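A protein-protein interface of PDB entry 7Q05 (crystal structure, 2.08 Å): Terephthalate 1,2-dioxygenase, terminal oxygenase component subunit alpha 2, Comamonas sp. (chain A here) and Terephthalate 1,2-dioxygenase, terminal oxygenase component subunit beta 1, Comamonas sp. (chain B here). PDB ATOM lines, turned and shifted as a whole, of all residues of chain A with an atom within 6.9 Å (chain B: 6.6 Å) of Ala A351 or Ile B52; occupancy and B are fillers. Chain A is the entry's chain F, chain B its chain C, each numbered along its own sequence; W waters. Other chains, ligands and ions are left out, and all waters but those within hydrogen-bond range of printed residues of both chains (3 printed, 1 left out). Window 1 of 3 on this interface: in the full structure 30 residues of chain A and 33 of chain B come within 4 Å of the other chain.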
ATOM      1  N   ARG A 191     -21.492  -6.547 -20.033  1.00  0.00           N
ATOM      2  CA  ARG A 191     -20.467  -6.642 -18.977  1.00  0.00           C
ATOM      3  C   ARG A 191     -19.295  -5.779 -19.420  1.00  0.00           C
ATOM      4  O   ARG A 191     -18.928  -5.851 -20.584  1.00  0.00           O
ATOM      5  CB  ARG A 191     -19.976  -8.075 -18.708  1.00  0.00           C
ATOM      6  CG  ARG A 191     -21.064  -9.009 -18.188  1.00  0.00           C
ATOM      7  CD  ARG A 191     -20.492 -10.383 -17.920  1.00  0.00           C
ATOM      8  NE  ARG A 191     -21.548 -11.265 -17.520  1.00  0.00           N
ATOM      9  CZ  ARG A 191     -22.316 -11.945 -18.353  1.00  0.00           C
ATOM     10  NH1 ARG A 191     -23.243 -12.731 -17.866  1.00  0.00           N
ATOM     11  NH2 ARG A 191     -22.167 -11.869 -19.658  1.00  0.00           N
ATOM     12  N   PHE A 192     -18.739  -5.021 -18.481  1.00  0.00           N
ATOM     13  CA  PHE A 192     -17.515  -4.220 -18.654  1.00  0.00           C
ATOM     14  C   PHE A 192     -16.817  -4.178 -17.311  1.00  0.00           C
ATOM     15  O   PHE A 192     -17.536  -4.107 -16.282  1.00  0.00           O
ATOM     16  CB  PHE A 192     -17.824  -2.797 -19.088  1.00  0.00           C
ATOM     17  CG  PHE A 192     -18.646  -2.719 -20.331  1.00  0.00           C
ATOM     18  CD1 PHE A 192     -18.055  -2.865 -21.568  1.00  0.00           C
ATOM     19  CD2 PHE A 192     -20.013  -2.518 -20.265  1.00  0.00           C
ATOM     20  CE1 PHE A 192     -18.807  -2.800 -22.714  1.00  0.00           C
ATOM     21  CE2 PHE A 192     -20.757  -2.426 -21.419  1.00  0.00           C
ATOM     22  CZ  PHE A 192     -20.149  -2.551 -22.635  1.00  0.00           C
ATOM     23  N   THR A 193     -15.485  -4.228 -17.359  1.00  0.00           N
ATOM     24  CA  THR A 193     -14.598  -4.136 -16.189  1.00  0.00           C
ATOM     25  C   THR A 193     -13.811  -2.835 -16.299  1.00  0.00           C
ATOM     26  O   THR A 193     -13.409  -2.462 -17.436  1.00  0.00           O
ATOM     27  CB  THR A 193     -13.651  -5.333 -16.169  1.00  0.00           C
ATOM     28  OG1 THR A 193     -14.488  -6.480 -15.993  1.00  0.00           O
ATOM     29  CG2 THR A 193     -12.576  -5.260 -15.101  1.00  0.00           C
ATOM     30  N   GLN A 194     -13.655  -2.140 -15.178  1.00  0.00           N
ATOM     31  CA  GLN A 194     -12.728  -0.994 -15.016  1.00  0.00           C
ATOM     32  C   GLN A 194     -11.605  -1.444 -14.086  1.00  0.00           C
ATOM     33  O   GLN A 194     -11.908  -1.937 -13.023  1.00  0.00           O
ATOM     34  CB  GLN A 194     -13.436   0.158 -14.320  1.00  0.00           C
ATOM     35  CG  GLN A 194     -14.019   1.128 -15.277  1.00  0.00           C
ATOM     36  CD  GLN A 194     -14.798   2.203 -14.576  1.00  0.00           C
ATOM     37  OE1 GLN A 194     -15.956   1.998 -14.296  1.00  0.00           O
ATOM     38  NE2 GLN A 194     -14.239   3.400 -14.462  1.00  0.00           N
ATOM     39  N   TYR A 327     -24.598  -4.804 -16.482  1.00  0.00           N
ATOM     40  CA  TYR A 327     -25.743  -3.961 -16.875  1.00  0.00           C
ATOM     41  C   TYR A 327     -26.973  -4.855 -17.002  1.00  0.00           C
ATOM     42  O   TYR A 327     -26.813  -6.025 -17.477  1.00  0.00           O
ATOM     43  CB  TYR A 327     -25.497  -3.251 -18.210  1.00  0.00           C
ATOM     44  CG  TYR A 327     -24.464  -2.158 -18.249  1.00  0.00           C
ATOM     45  CD1 TYR A 327     -23.480  -2.013 -17.304  1.00  0.00           C
ATOM     46  CD2 TYR A 327     -24.422  -1.308 -19.336  1.00  0.00           C
ATOM     47  CE1 TYR A 327     -22.492  -1.043 -17.412  1.00  0.00           C
ATOM     48  CE2 TYR A 327     -23.426  -0.363 -19.481  1.00  0.00           C
ATOM     49  CZ  TYR A 327     -22.469  -0.195 -18.498  1.00  0.00           C
ATOM     50  OH  TYR A 327     -21.512   0.773 -18.661  1.00  0.00           O
ATOM     51  N   ALA A 345     -27.746   4.059 -20.297  1.00  0.00           N
ATOM     52  CA  ALA A 345     -26.465   3.446 -19.874  1.00  0.00           C
ATOM     53  C   ALA A 345     -25.295   4.412 -20.121  1.00  0.00           C
ATOM     54  O   ALA A 345     -24.239   4.220 -19.513  1.00  0.00           O
ATOM     55  CB  ALA A 345     -26.261   2.129 -20.593  1.00  0.00           C
ATOM     56  N   ASN A 346     -25.467   5.404 -20.994  1.00  0.00           N
ATOM     57  CA  ASN A 346     -24.421   6.428 -21.255  1.00  0.00           C
ATOM     58  C   ASN A 346     -24.088   7.177 -19.964  1.00  0.00           C
ATOM     59  O   ASN A 346     -22.996   7.797 -19.933  1.00  0.00           O
ATOM     60  CB  ASN A 346     -24.809   7.372 -22.383  1.00  0.00           C
ATOM     61  CG  ASN A 346     -24.722   6.687 -23.739  1.00  0.00           C
ATOM     62  OD1 ASN A 346     -23.655   6.422 -24.257  1.00  0.00           O
ATOM     63  ND2 ASN A 346     -25.836   6.399 -24.341  1.00  0.00           N
ATOM     64  N   LEU A 347     -24.974   7.113 -18.944  1.00  0.00           N
ATOM     65  CA  LEU A 347     -24.793   7.870 -17.685  1.00  0.00           C
ATOM     66  C   LEU A 347     -23.768   7.159 -16.831  1.00  0.00           C
ATOM     67  O   LEU A 347     -23.167   7.818 -15.980  1.00  0.00           O
ATOM     68  CB  LEU A 347     -26.127   7.977 -16.957  1.00  0.00           C
ATOM     69  CG  LEU A 347     -27.184   8.792 -17.695  1.00  0.00           C
ATOM     70  CD1 LEU A 347     -28.541   8.691 -17.004  1.00  0.00           C
ATOM     71  CD2 LEU A 347     -26.746  10.243 -17.782  1.00  0.00           C
ATOM     72  N   ILE A 348     -23.615   5.849 -17.029  1.00  0.00           N
ATOM     73  CA  ILE A 348     -22.901   4.951 -16.064  1.00  0.00           C
ATOM     74  C   ILE A 348     -21.725   4.285 -16.779  1.00  0.00           C
ATOM     75  O   ILE A 348     -21.561   4.383 -18.002  1.00  0.00           O
ATOM     76  CB  ILE A 348     -23.849   3.869 -15.489  1.00  0.00           C
ATOM     77  CG1 ILE A 348     -24.298   2.874 -16.573  1.00  0.00           C
ATOM     78  CG2 ILE A 348     -25.060   4.516 -14.826  1.00  0.00           C
ATOM     79  CD1 ILE A 348     -24.834   1.568 -16.075  1.00  0.00           C
ATOM     80  N   GLY A 349     -20.958   3.557 -16.015  1.00  0.00           N
ATOM     81  CA  GLY A 349     -19.853   2.754 -16.536  1.00  0.00           C
ATOM     82  C   GLY A 349     -18.616   3.598 -16.774  1.00  0.00           C
ATOM     83  O   GLY A 349     -18.509   4.760 -16.333  1.00  0.00           O
ATOM     84  N   PRO A 350     -17.642   2.985 -17.468  1.00  0.00           N
ATOM     85  CA  PRO A 350     -16.317   3.572 -17.669  1.00  0.00           C
ATOM     86  C   PRO A 350     -16.296   4.954 -18.301  1.00  0.00           C
ATOM     87  O   PRO A 350     -15.380   5.634 -18.051  1.00  0.00           O
ATOM     88  CB  PRO A 350     -15.667   2.576 -18.636  1.00  0.00           C
ATOM     89  CG  PRO A 350     -16.305   1.270 -18.265  1.00  0.00           C
ATOM     90  CD  PRO A 350     -17.745   1.623 -17.996  1.00  0.00           C
ATOM     91  N   ALA A 351     -17.274   5.246 -19.167  1.00  0.00           N
ATOM     92  CA  ALA A 351     -17.421   6.500 -19.913  1.00  0.00           C
ATOM     93  C   ALA A 351     -18.697   7.226 -19.473  1.00  0.00           C
ATOM     94  O   ALA A 351     -19.227   8.006 -20.236  1.00  0.00           O
ATOM     95  CB  ALA A 351     -17.447   6.164 -21.383  1.00  0.00           C
ATOM     96  N   GLY A 352     -19.233   6.940 -18.299  1.00  0.00           N
ATOM     97  CA  GLY A 352     -20.545   7.500 -17.875  1.00  0.00           C
ATOM     98  C   GLY A 352     -20.515   9.001 -17.706  1.00  0.00           C
ATOM     99  O   GLY A 352     -19.600   9.487 -17.063  1.00  0.00           O
ATOM    100  N   PHE A 353     -21.486   9.722 -18.236  1.00  0.00           N
ATOM    101  CA  PHE A 353     -21.658  11.169 -17.952  1.00  0.00           C
ATOM    102  C   PHE A 353     -21.588  11.453 -16.435  1.00  0.00           C
ATOM    103  O   PHE A 353     -21.082  12.536 -16.018  1.00  0.00           O
ATOM    104  CB  PHE A 353     -22.972  11.664 -18.548  1.00  0.00           C
ATOM    105  CG  PHE A 353     -23.028  11.545 -20.052  1.00  0.00           C
ATOM    106  CD1 PHE A 353     -21.938  11.902 -20.829  1.00  0.00           C
ATOM    107  CD2 PHE A 353     -24.182  11.117 -20.688  1.00  0.00           C
ATOM    108  CE1 PHE A 353     -21.997  11.795 -22.205  1.00  0.00           C
ATOM    109  CE2 PHE A 353     -24.234  11.014 -22.070  1.00  0.00           C
ATOM    110  CZ  PHE A 353     -23.129  11.310 -22.821  1.00  0.00           C
ATOM    111  N   ILE A 354     -22.104  10.529 -15.627  1.00  0.00           N
ATOM    112  CA  ILE A 354     -22.070  10.603 -14.143  1.00  0.00           C
ATOM    113  C   ILE A 354     -20.845   9.837 -13.628  1.00  0.00           C
ATOM    114  O   ILE A 354     -20.085  10.401 -12.875  1.00  0.00           O
ATOM    115  CB  ILE A 354     -23.379  10.079 -13.510  1.00  0.00           C
ATOM    116  CG1 ILE A 354     -24.578  10.971 -13.846  1.00  0.00           C
ATOM    117  CG2 ILE A 354     -23.212   9.889 -12.002  1.00  0.00           C
ATOM    118  CD1 ILE A 354     -25.917  10.265 -13.650  1.00  0.00           C
ATOM    119  N   SER A 355     -20.650   8.583 -13.988  1.00  0.00           N
ATOM    120  CA  SER A 355     -19.683   7.736 -13.249  1.00  0.00           C
ATOM    121  C   SER A 355     -18.233   7.855 -13.747  1.00  0.00           C
ATOM    122  O   SER A 355     -17.372   7.166 -13.139  1.00  0.00           O
ATOM    123  CB  SER A 355     -20.158   6.315 -13.207  1.00  0.00           C
ATOM    124  OG  SER A 355     -20.499   5.914 -14.486  1.00  0.00           O
ATOM    125  N   MET A 356     -17.965   8.577 -14.839  1.00  0.00           N
ATOM    126  CA  MET A 356     -16.628   8.578 -15.504  1.00  0.00           C
ATOM    127  C   MET A 356     -15.562   8.934 -14.455  1.00  0.00           C
ATOM    128  O   MET A 356     -14.619   8.195 -14.279  1.00  0.00           O
ATOM    129  CB  MET A 356     -16.627   9.617 -16.622  1.00  0.00           C
ATOM    130  CG  MET A 356     -15.330   9.662 -17.366  1.00  0.00           C
ATOM    131  SD  MET A 356     -15.194  10.935 -18.611  1.00  0.00           S
ATOM    132  CE  MET A 356     -16.594  10.509 -19.656  1.00  0.00           C
ATOM    133  N   ARG B  37     -21.201   2.440 -31.033  1.00  0.00           N
ATOM    134  CA  ARG B  37     -21.146   1.647 -29.782  1.00  0.00           C
ATOM    135  C   ARG B  37     -19.713   1.237 -29.530  1.00  0.00           C
ATOM    136  O   ARG B  37     -19.042   0.825 -30.497  1.00  0.00           O
ATOM    137  CB  ARG B  37     -21.958   0.380 -29.989  1.00  0.00           C
ATOM    138  CG  ARG B  37     -22.456  -0.307 -28.748  1.00  0.00           C
ATOM    139  CD  ARG B  37     -23.588  -1.159 -29.282  1.00  0.00           C
ATOM    140  NE  ARG B  37     -23.286  -2.555 -29.503  1.00  0.00           N
ATOM    141  CZ  ARG B  37     -23.680  -3.217 -30.567  1.00  0.00           C
ATOM    142  NH1 ARG B  37     -23.371  -4.476 -30.683  1.00  0.00           N
ATOM    143  NH2 ARG B  37     -24.254  -2.615 -31.589  1.00  0.00           N
ATOM    144  N   VAL B  38     -19.307   1.287 -28.267  1.00  0.00           N
ATOM    145  CA  VAL B  38     -18.037   0.687 -27.786  1.00  0.00           C
ATOM    146  C   VAL B  38     -18.439  -0.514 -26.945  1.00  0.00           C
ATOM    147  O   VAL B  38     -19.179  -0.328 -25.966  1.00  0.00           O
ATOM    148  CB  VAL B  38     -17.189   1.674 -26.976  1.00  0.00           C
ATOM    149  CG1 VAL B  38     -15.986   0.962 -26.381  1.00  0.00           C
ATOM    150  CG2 VAL B  38     -16.769   2.885 -27.819  1.00  0.00           C
ATOM    151  N   THR B  39     -17.974  -1.701 -27.338  1.00  0.00           N
ATOM    152  CA  THR B  39     -18.315  -2.967 -26.674  1.00  0.00           C
ATOM    153  C   THR B  39     -17.075  -3.825 -26.647  1.00  0.00           C
ATOM    154  O   THR B  39     -15.957  -3.266 -26.787  1.00  0.00           O
ATOM    155  CB  THR B  39     -19.547  -3.611 -27.291  1.00  0.00           C
ATOM    156  OG1 THR B  39     -19.913  -4.622 -26.348  1.00  0.00           O
ATOM    157  CG2 THR B  39     -19.271  -4.124 -28.687  1.00  0.00           C
ATOM    158  N   ASN B  40     -17.251  -5.114 -26.343  1.00  0.00           N
ATOM    159  CA  ASN B  40     -16.096  -6.047 -26.267  1.00  0.00           C
ATOM    160  C   ASN B  40     -16.501  -7.361 -26.907  1.00  0.00           C
ATOM    161  O   ASN B  40     -17.707  -7.531 -27.152  1.00  0.00           O
ATOM    162  CB  ASN B  40     -15.562  -6.163 -24.847  1.00  0.00           C
ATOM    163  CG  ASN B  40     -16.617  -6.616 -23.868  1.00  0.00           C
ATOM    164  OD1 ASN B  40     -17.286  -7.638 -24.095  1.00  0.00           O
ATOM    165  ND2 ASN B  40     -16.736  -5.895 -22.758  1.00  0.00           N
ATOM    166  N   ALA B  50     -25.482  -3.634 -24.956  1.00  0.00           N
ATOM    167  CA  ALA B  50     -25.029  -2.411 -24.252  1.00  0.00           C
ATOM    168  C   ALA B  50     -23.640  -1.998 -24.722  1.00  0.00           C
ATOM    169  O   ALA B  50     -22.829  -2.879 -25.072  1.00  0.00           O
ATOM    170  CB  ALA B  50     -25.015  -2.580 -22.717  1.00  0.00           C
ATOM    171  N   GLY B  51     -23.372  -0.697 -24.682  1.00  0.00           N
ATOM    172  CA  GLY B  51     -22.038  -0.140 -24.947  1.00  0.00           C
ATOM    173  C   GLY B  51     -21.645   0.779 -23.807  1.00  0.00           C
ATOM    174  O   GLY B  51     -22.520   1.375 -23.147  1.00  0.00           O
ATOM    175  N   ILE B  52     -20.354   0.863 -23.562  1.00  0.00           N
ATOM    176  CA  ILE B  52     -19.725   1.912 -22.706  1.00  0.00           C
ATOM    177  C   ILE B  52     -20.161   3.283 -23.279  1.00  0.00           C
ATOM    178  O   ILE B  52     -20.399   4.255 -22.519  1.00  0.00           O
ATOM    179  CB  ILE B  52     -18.208   1.672 -22.773  1.00  0.00           C
ATOM    180  CG1 ILE B  52     -17.772   0.509 -21.889  1.00  0.00           C
ATOM    181  CG2 ILE B  52     -17.424   2.900 -22.452  1.00  0.00           C
ATOM    182  CD1 ILE B  52     -16.307   0.113 -22.209  1.00  0.00           C
ATOM    183  N   VAL B  53     -20.232   3.349 -24.605  1.00  0.00           N
ATOM    184  CA  VAL B  53     -20.864   4.457 -25.371  1.00  0.00           C
ATOM    185  C   VAL B  53     -21.894   3.777 -26.254  1.00  0.00           C
ATOM    186  O   VAL B  53     -21.574   2.691 -26.768  1.00  0.00           O
ATOM    187  CB  VAL B  53     -19.862   5.235 -26.251  1.00  0.00           C
ATOM    188  CG1 VAL B  53     -20.571   6.375 -26.981  1.00  0.00           C
ATOM    189  CG2 VAL B  53     -18.667   5.737 -25.454  1.00  0.00           C
ATOM    190  N   TRP B  54     -23.083   4.379 -26.360  1.00  0.00           N
ATOM    191  CA  TRP B  54     -24.192   3.832 -27.162  1.00  0.00           C
ATOM    192  C   TRP B  54     -24.928   5.014 -27.748  1.00  0.00           C
ATOM    193  O   TRP B  54     -25.426   5.787 -26.974  1.00  0.00           O
ATOM    194  CB  TRP B  54     -25.117   2.967 -26.314  1.00  0.00           C
ATOM    195  CG  TRP B  54     -26.047   2.101 -27.116  1.00  0.00           C
ATOM    196  CD1 TRP B  54     -25.910   0.769 -27.333  1.00  0.00           C
ATOM    197  CD2 TRP B  54     -27.299   2.473 -27.713  1.00  0.00           C
ATOM    198  NE1 TRP B  54     -26.985   0.287 -28.026  1.00  0.00           N
ATOM    199  CE2 TRP B  54     -27.848   1.307 -28.286  1.00  0.00           C
ATOM    200  CE3 TRP B  54     -28.001   3.668 -27.833  1.00  0.00           C
ATOM    201  CZ2 TRP B  54     -29.034   1.307 -29.033  1.00  0.00           C
ATOM    202  CZ3 TRP B  54     -29.172   3.679 -28.561  1.00  0.00           C
ATOM    203  CH2 TRP B  54     -29.683   2.517 -29.158  1.00  0.00           C
ATOM    204  N   ARG B  64     -22.247  14.085 -26.345  1.00  0.00           N
ATOM    205  CA  ARG B  64     -21.157  13.398 -25.594  1.00  0.00           C
ATOM    206  C   ARG B  64     -19.907  14.286 -25.640  1.00  0.00           C
ATOM    207  O   ARG B  64     -19.227  14.379 -24.594  1.00  0.00           O
ATOM    208  CB  ARG B  64     -20.934  11.975 -26.096  1.00  0.00           C
ATOM    209  CG  ARG B  64     -19.735  11.273 -25.486  1.00  0.00           C
ATOM    210  CD  ARG B  64     -19.711   9.761 -25.732  1.00  0.00           C
ATOM    211  NE  ARG B  64     -20.603   9.053 -24.836  1.00  0.00           N
ATOM    212  CZ  ARG B  64     -20.341   8.733 -23.569  1.00  0.00           C
ATOM    213  NH1 ARG B  64     -19.203   9.094 -23.011  1.00  0.00           N
ATOM    214  NH2 ARG B  64     -21.242   8.069 -22.845  1.00  0.00           N
ATOM    215  N   ASN B  72     -17.296  16.751 -17.740  1.00  0.00           N
ATOM    216  CA  ASN B  72     -16.535  15.564 -17.280  1.00  0.00           C
ATOM    217  C   ASN B  72     -15.154  15.984 -16.748  1.00  0.00           C
ATOM    218  O   ASN B  72     -14.582  16.966 -17.274  1.00  0.00           O
ATOM    219  CB  ASN B  72     -16.518  14.492 -18.363  1.00  0.00           C
ATOM    220  CG  ASN B  72     -17.882  13.845 -18.566  1.00  0.00           C
ATOM    221  OD1 ASN B  72     -18.215  13.497 -19.681  1.00  0.00           O
ATOM    222  ND2 ASN B  72     -18.678  13.669 -17.515  1.00  0.00           N
ATOM    223  N   CYS B 141     -13.956  -4.163 -28.745  1.00  0.00           N
ATOM    224  CA  CYS B 141     -12.656  -4.263 -28.013  1.00  0.00           C
ATOM    225  C   CYS B 141     -12.327  -5.737 -27.728  1.00  0.00           C
ATOM    226  O   CYS B 141     -13.224  -6.509 -27.398  1.00  0.00           O
ATOM    227  CB  CYS B 141     -12.674  -3.402 -26.760  1.00  0.00           C
ATOM    228  SG  CYS B 141     -12.817  -1.640 -27.160  1.00  0.00           S
ATOM    229  N   THR B 144     -12.199  -6.988 -22.119  1.00  0.00           N
ATOM    230  CA  THR B 144     -13.328  -6.547 -21.260  1.00  0.00           C
ATOM    231  C   THR B 144     -12.866  -5.450 -20.280  1.00  0.00           C
ATOM    232  O   THR B 144     -13.720  -4.899 -19.564  1.00  0.00           O
ATOM    233  CB  THR B 144     -13.877  -7.769 -20.517  1.00  0.00           C
ATOM    234  OG1 THR B 144     -12.790  -8.425 -19.852  1.00  0.00           O
ATOM    235  CG2 THR B 144     -14.476  -8.765 -21.482  1.00  0.00           C
ATOM    236  N   THR B 146     -11.192  -1.749 -19.324  1.00  0.00           N
ATOM    237  CA  THR B 146     -10.822  -0.349 -19.555  1.00  0.00           C
ATOM    238  C   THR B 146      -9.998   0.100 -18.355  1.00  0.00           C
ATOM    239  O   THR B 146     -10.469   0.005 -17.212  1.00  0.00           O
ATOM    240  CB  THR B 146     -12.053   0.545 -19.686  1.00  0.00           C
ATOM    241  OG1 THR B 146     -12.880   0.062 -20.733  1.00  0.00           O
ATOM    242  CG2 THR B 146     -11.677   1.988 -19.944  1.00  0.00           C
ATOM    243  N   LEU B 149     -10.809   4.789 -16.771  1.00  0.00           N
ATOM    244  CA  LEU B 149     -12.061   5.346 -17.368  1.00  0.00           C
ATOM    245  C   LEU B 149     -11.843   5.466 -18.880  1.00  0.00           C
ATOM    246  O   LEU B 149     -10.714   5.259 -19.333  1.00  0.00           O
ATOM    247  CB  LEU B 149     -12.414   6.700 -16.749  1.00  0.00           C
ATOM    248  CG  LEU B 149     -11.317   7.776 -16.841  1.00  0.00           C
ATOM    249  CD1 LEU B 149     -11.268   8.403 -18.227  1.00  0.00           C
ATOM    250  CD2 LEU B 149     -11.515   8.865 -15.819  1.00  0.00           C
ATOM    251  N   MET B 150     -12.904   5.785 -19.620  1.00  0.00           N
ATOM    252  CA  MET B 150     -12.859   6.074 -21.073  1.00  0.00           C
ATOM    253  C   MET B 150     -13.526   7.426 -21.306  1.00  0.00           C
ATOM    254  O   MET B 150     -14.773   7.545 -21.134  1.00  0.00           O
ATOM    255  CB  MET B 150     -13.552   4.985 -21.880  1.00  0.00           C
ATOM    256  CG  MET B 150     -13.389   5.214 -23.406  1.00  0.00           C
ATOM    257  SD  MET B 150     -14.032   3.968 -24.482  1.00  0.00           S
ATOM    258  CE  MET B 150     -12.961   2.595 -24.082  1.00  0.00           C
ATOM    259  N   ALA B 151     -12.737   8.444 -21.636  1.00  0.00           N
ATOM    260  CA  ALA B 151     -13.236   9.833 -21.819  1.00  0.00           C
ATOM    261  C   ALA B 151     -13.430  10.081 -23.317  1.00  0.00           C
ATOM    262  O   ALA B 151     -14.411  10.612 -23.713  1.00  0.00           O
ATOM    263  CB  ALA B 151     -12.276  10.840 -21.239  1.00  0.00           C
HETATM  264  O   HOH W   1     -14.469  -2.035 -20.041  1.00  0.00           O
HETATM  265  O   HOH W   2     -23.389   8.912 -25.993  1.00  0.00           O
HETATM  266  O   HOH W   3     -19.677   3.854 -19.865  1.00  0.00           O
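CA of Thr B39 touches CE1 of Phe A192, 3.99 Å away.
Ile B52 touches Phe A192.
Phe A192 touches Thr B144 (C to O, 3.9 Å).
CA of Gln A194 touches O of Thr B146, 3.3 Å away.
CA of Leu B149 touches O of Pro A350, 3.4 Å away.
CG2 of Ile B52 touches CB of Ala A351, 3.4 Å away.
Ala A351 touches Met B150.
Met A356 touches Asn B72.
Met A356 touches Met B150 (CE to O, 3.8 Å).
CA of Ala B151 touches SD of Met A356, at 3.9 Å.
Printed residues of chain B that touch a printed residue of chain A: Thr B39, Asn B40, Ala B50, Gly B51, Ile B52, Val B53, Trp B54, Arg B64, Asn B72, Thr B144, Thr B146, Leu B149, Met B150 and Ala B151.
Of the 17 printed residues of chain A, 10 touch a printed residue of chain B.
Printed residues of chain A that touch a printed residue of chain B: Arg A191, Phe A192, Thr A193, Gln A194, Tyr A327, Asn A346, Pro A350, Ala A351, Phe A353 and Met A356.
Hydrophobic or aromatic side chains of chain A within 4 Å of the printed part of chain B: Phe A192, Tyr A327, Pro A350, Ala A351, Phe A353 and Met A356.
Among the printed residues, no Asp or Glu carboxylate lies within 4 Å of a Lys or Arg side-chain nitrogen of the other chain.
O of Ala A351 lies within hydrogen-bond range of NH1 of Arg B64.
NH2 of Arg B64 sits at hydrogen-bond distance from OD1 of Asn A346 (3.2 Å).
The backbone carbonyl oxygen (O) of Pro A350 sits at hydrogen-bond distance from the backbone NH (N) of Met B150, at 2.9 Å.
N of Thr B146 is in hydrogen-bond range of O of Thr A193, at 3.0 Å.
The backbone carbonyl oxygen (O) of Arg A191 is in hydrogen-bond range of the side-chain amide nitrogen (ND2) of Asn B40 (3.1 Å).
The backbone carbonyl oxygen (O) of Thr B144 lies within hydrogen-bond range of the backbone NH (N) of Thr A193 (2.9 Å).
The backbone carbonyl oxygen (O) of Trp B54 sits at hydrogen-bond distance from the side-chain amide nitrogen (ND2) of Asn A346 (2.7 Å).
The backbone carbonyl oxygen (O) of Phe A353 lies within hydrogen-bond range of the side-chain amide nitrogen (ND2) of Asn B72 (3.1 Å).
The backbone carbonyl oxygen (O) of Asn A346 lies within hydrogen-bond range of the backbone NH (N) of Phe A353, 3.0 Å away.
The backbone NH (N) of Ile B52 sits at hydrogen-bond distance from the backbone carbonyl oxygen (O) of Val B38 (2.9 Å).
The backbone carbonyl oxygen of Val B53 sits at hydrogen-bond distance from the backbone NH of Val B38 (3.1 Å).
The backbone carbonyl oxygen of Leu A347 sits at hydrogen-bond distance from the backbone NH of Phe A353 (3.4 Å).
The backbone carbonyl oxygen (O) of Thr B39 is in hydrogen-bond range of the backbone NH (N) of Cys B141 (2.9 Å).
Printed residues of chain B within 4 Å of Gln A194: Thr B146 (3.3 Å).
Printed residues of chain B within 4 Å of Tyr A327: Ala B50 (3.7 Å).
Of the printed residues of chain B, Pro A350 touches Ile B52, Leu B149 and Met B150.
Ala A351 touches just these residues of chain B: Ile B52, Arg B64 and Met B150.
Of the printed residues of chain A, Ile B52 touches Phe A192 (3.4 Å), Pro A350 (3.98 Å) and Ala A351 (3.4 Å).
Of the printed residues of chain A, Thr B144 touches Phe A192 (3.9 Å) and Thr A193 (2.9 Å).
Of the printed residues of chain A, Leu B149 touches Pro A350 and Met A356.
The nearest printed residue of chain A that does not touch Ile B52 is Asn A346 (4.3 Å).
The nearest printed residue of chain B that does not touch Tyr A327 is Gly B51 (4.2 Å).
Water W3 lies within hydrogen-bond range of the backbone carbonyl oxygen (O) of Ile A348 (2.7 Å), the backbone carbonyl oxygen (O) of Ile B52 (2.8 Å), the backbone NH (N) of Ala A351 (2.9 Å) and the backbone NH (N) of Gly A352 (3.5 Å).
Water W1 lies within hydrogen-bond range of OG1 of Thr B146 (2.7 Å), O of Thr A193 (2.8 Å) and O of Thr B144 (3.0 Å).
Water W2 bridges the guanidinium group of Arg B64 (3.0 Å) and the side-chain amide oxygen of Asn A346 (3.0 Å).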
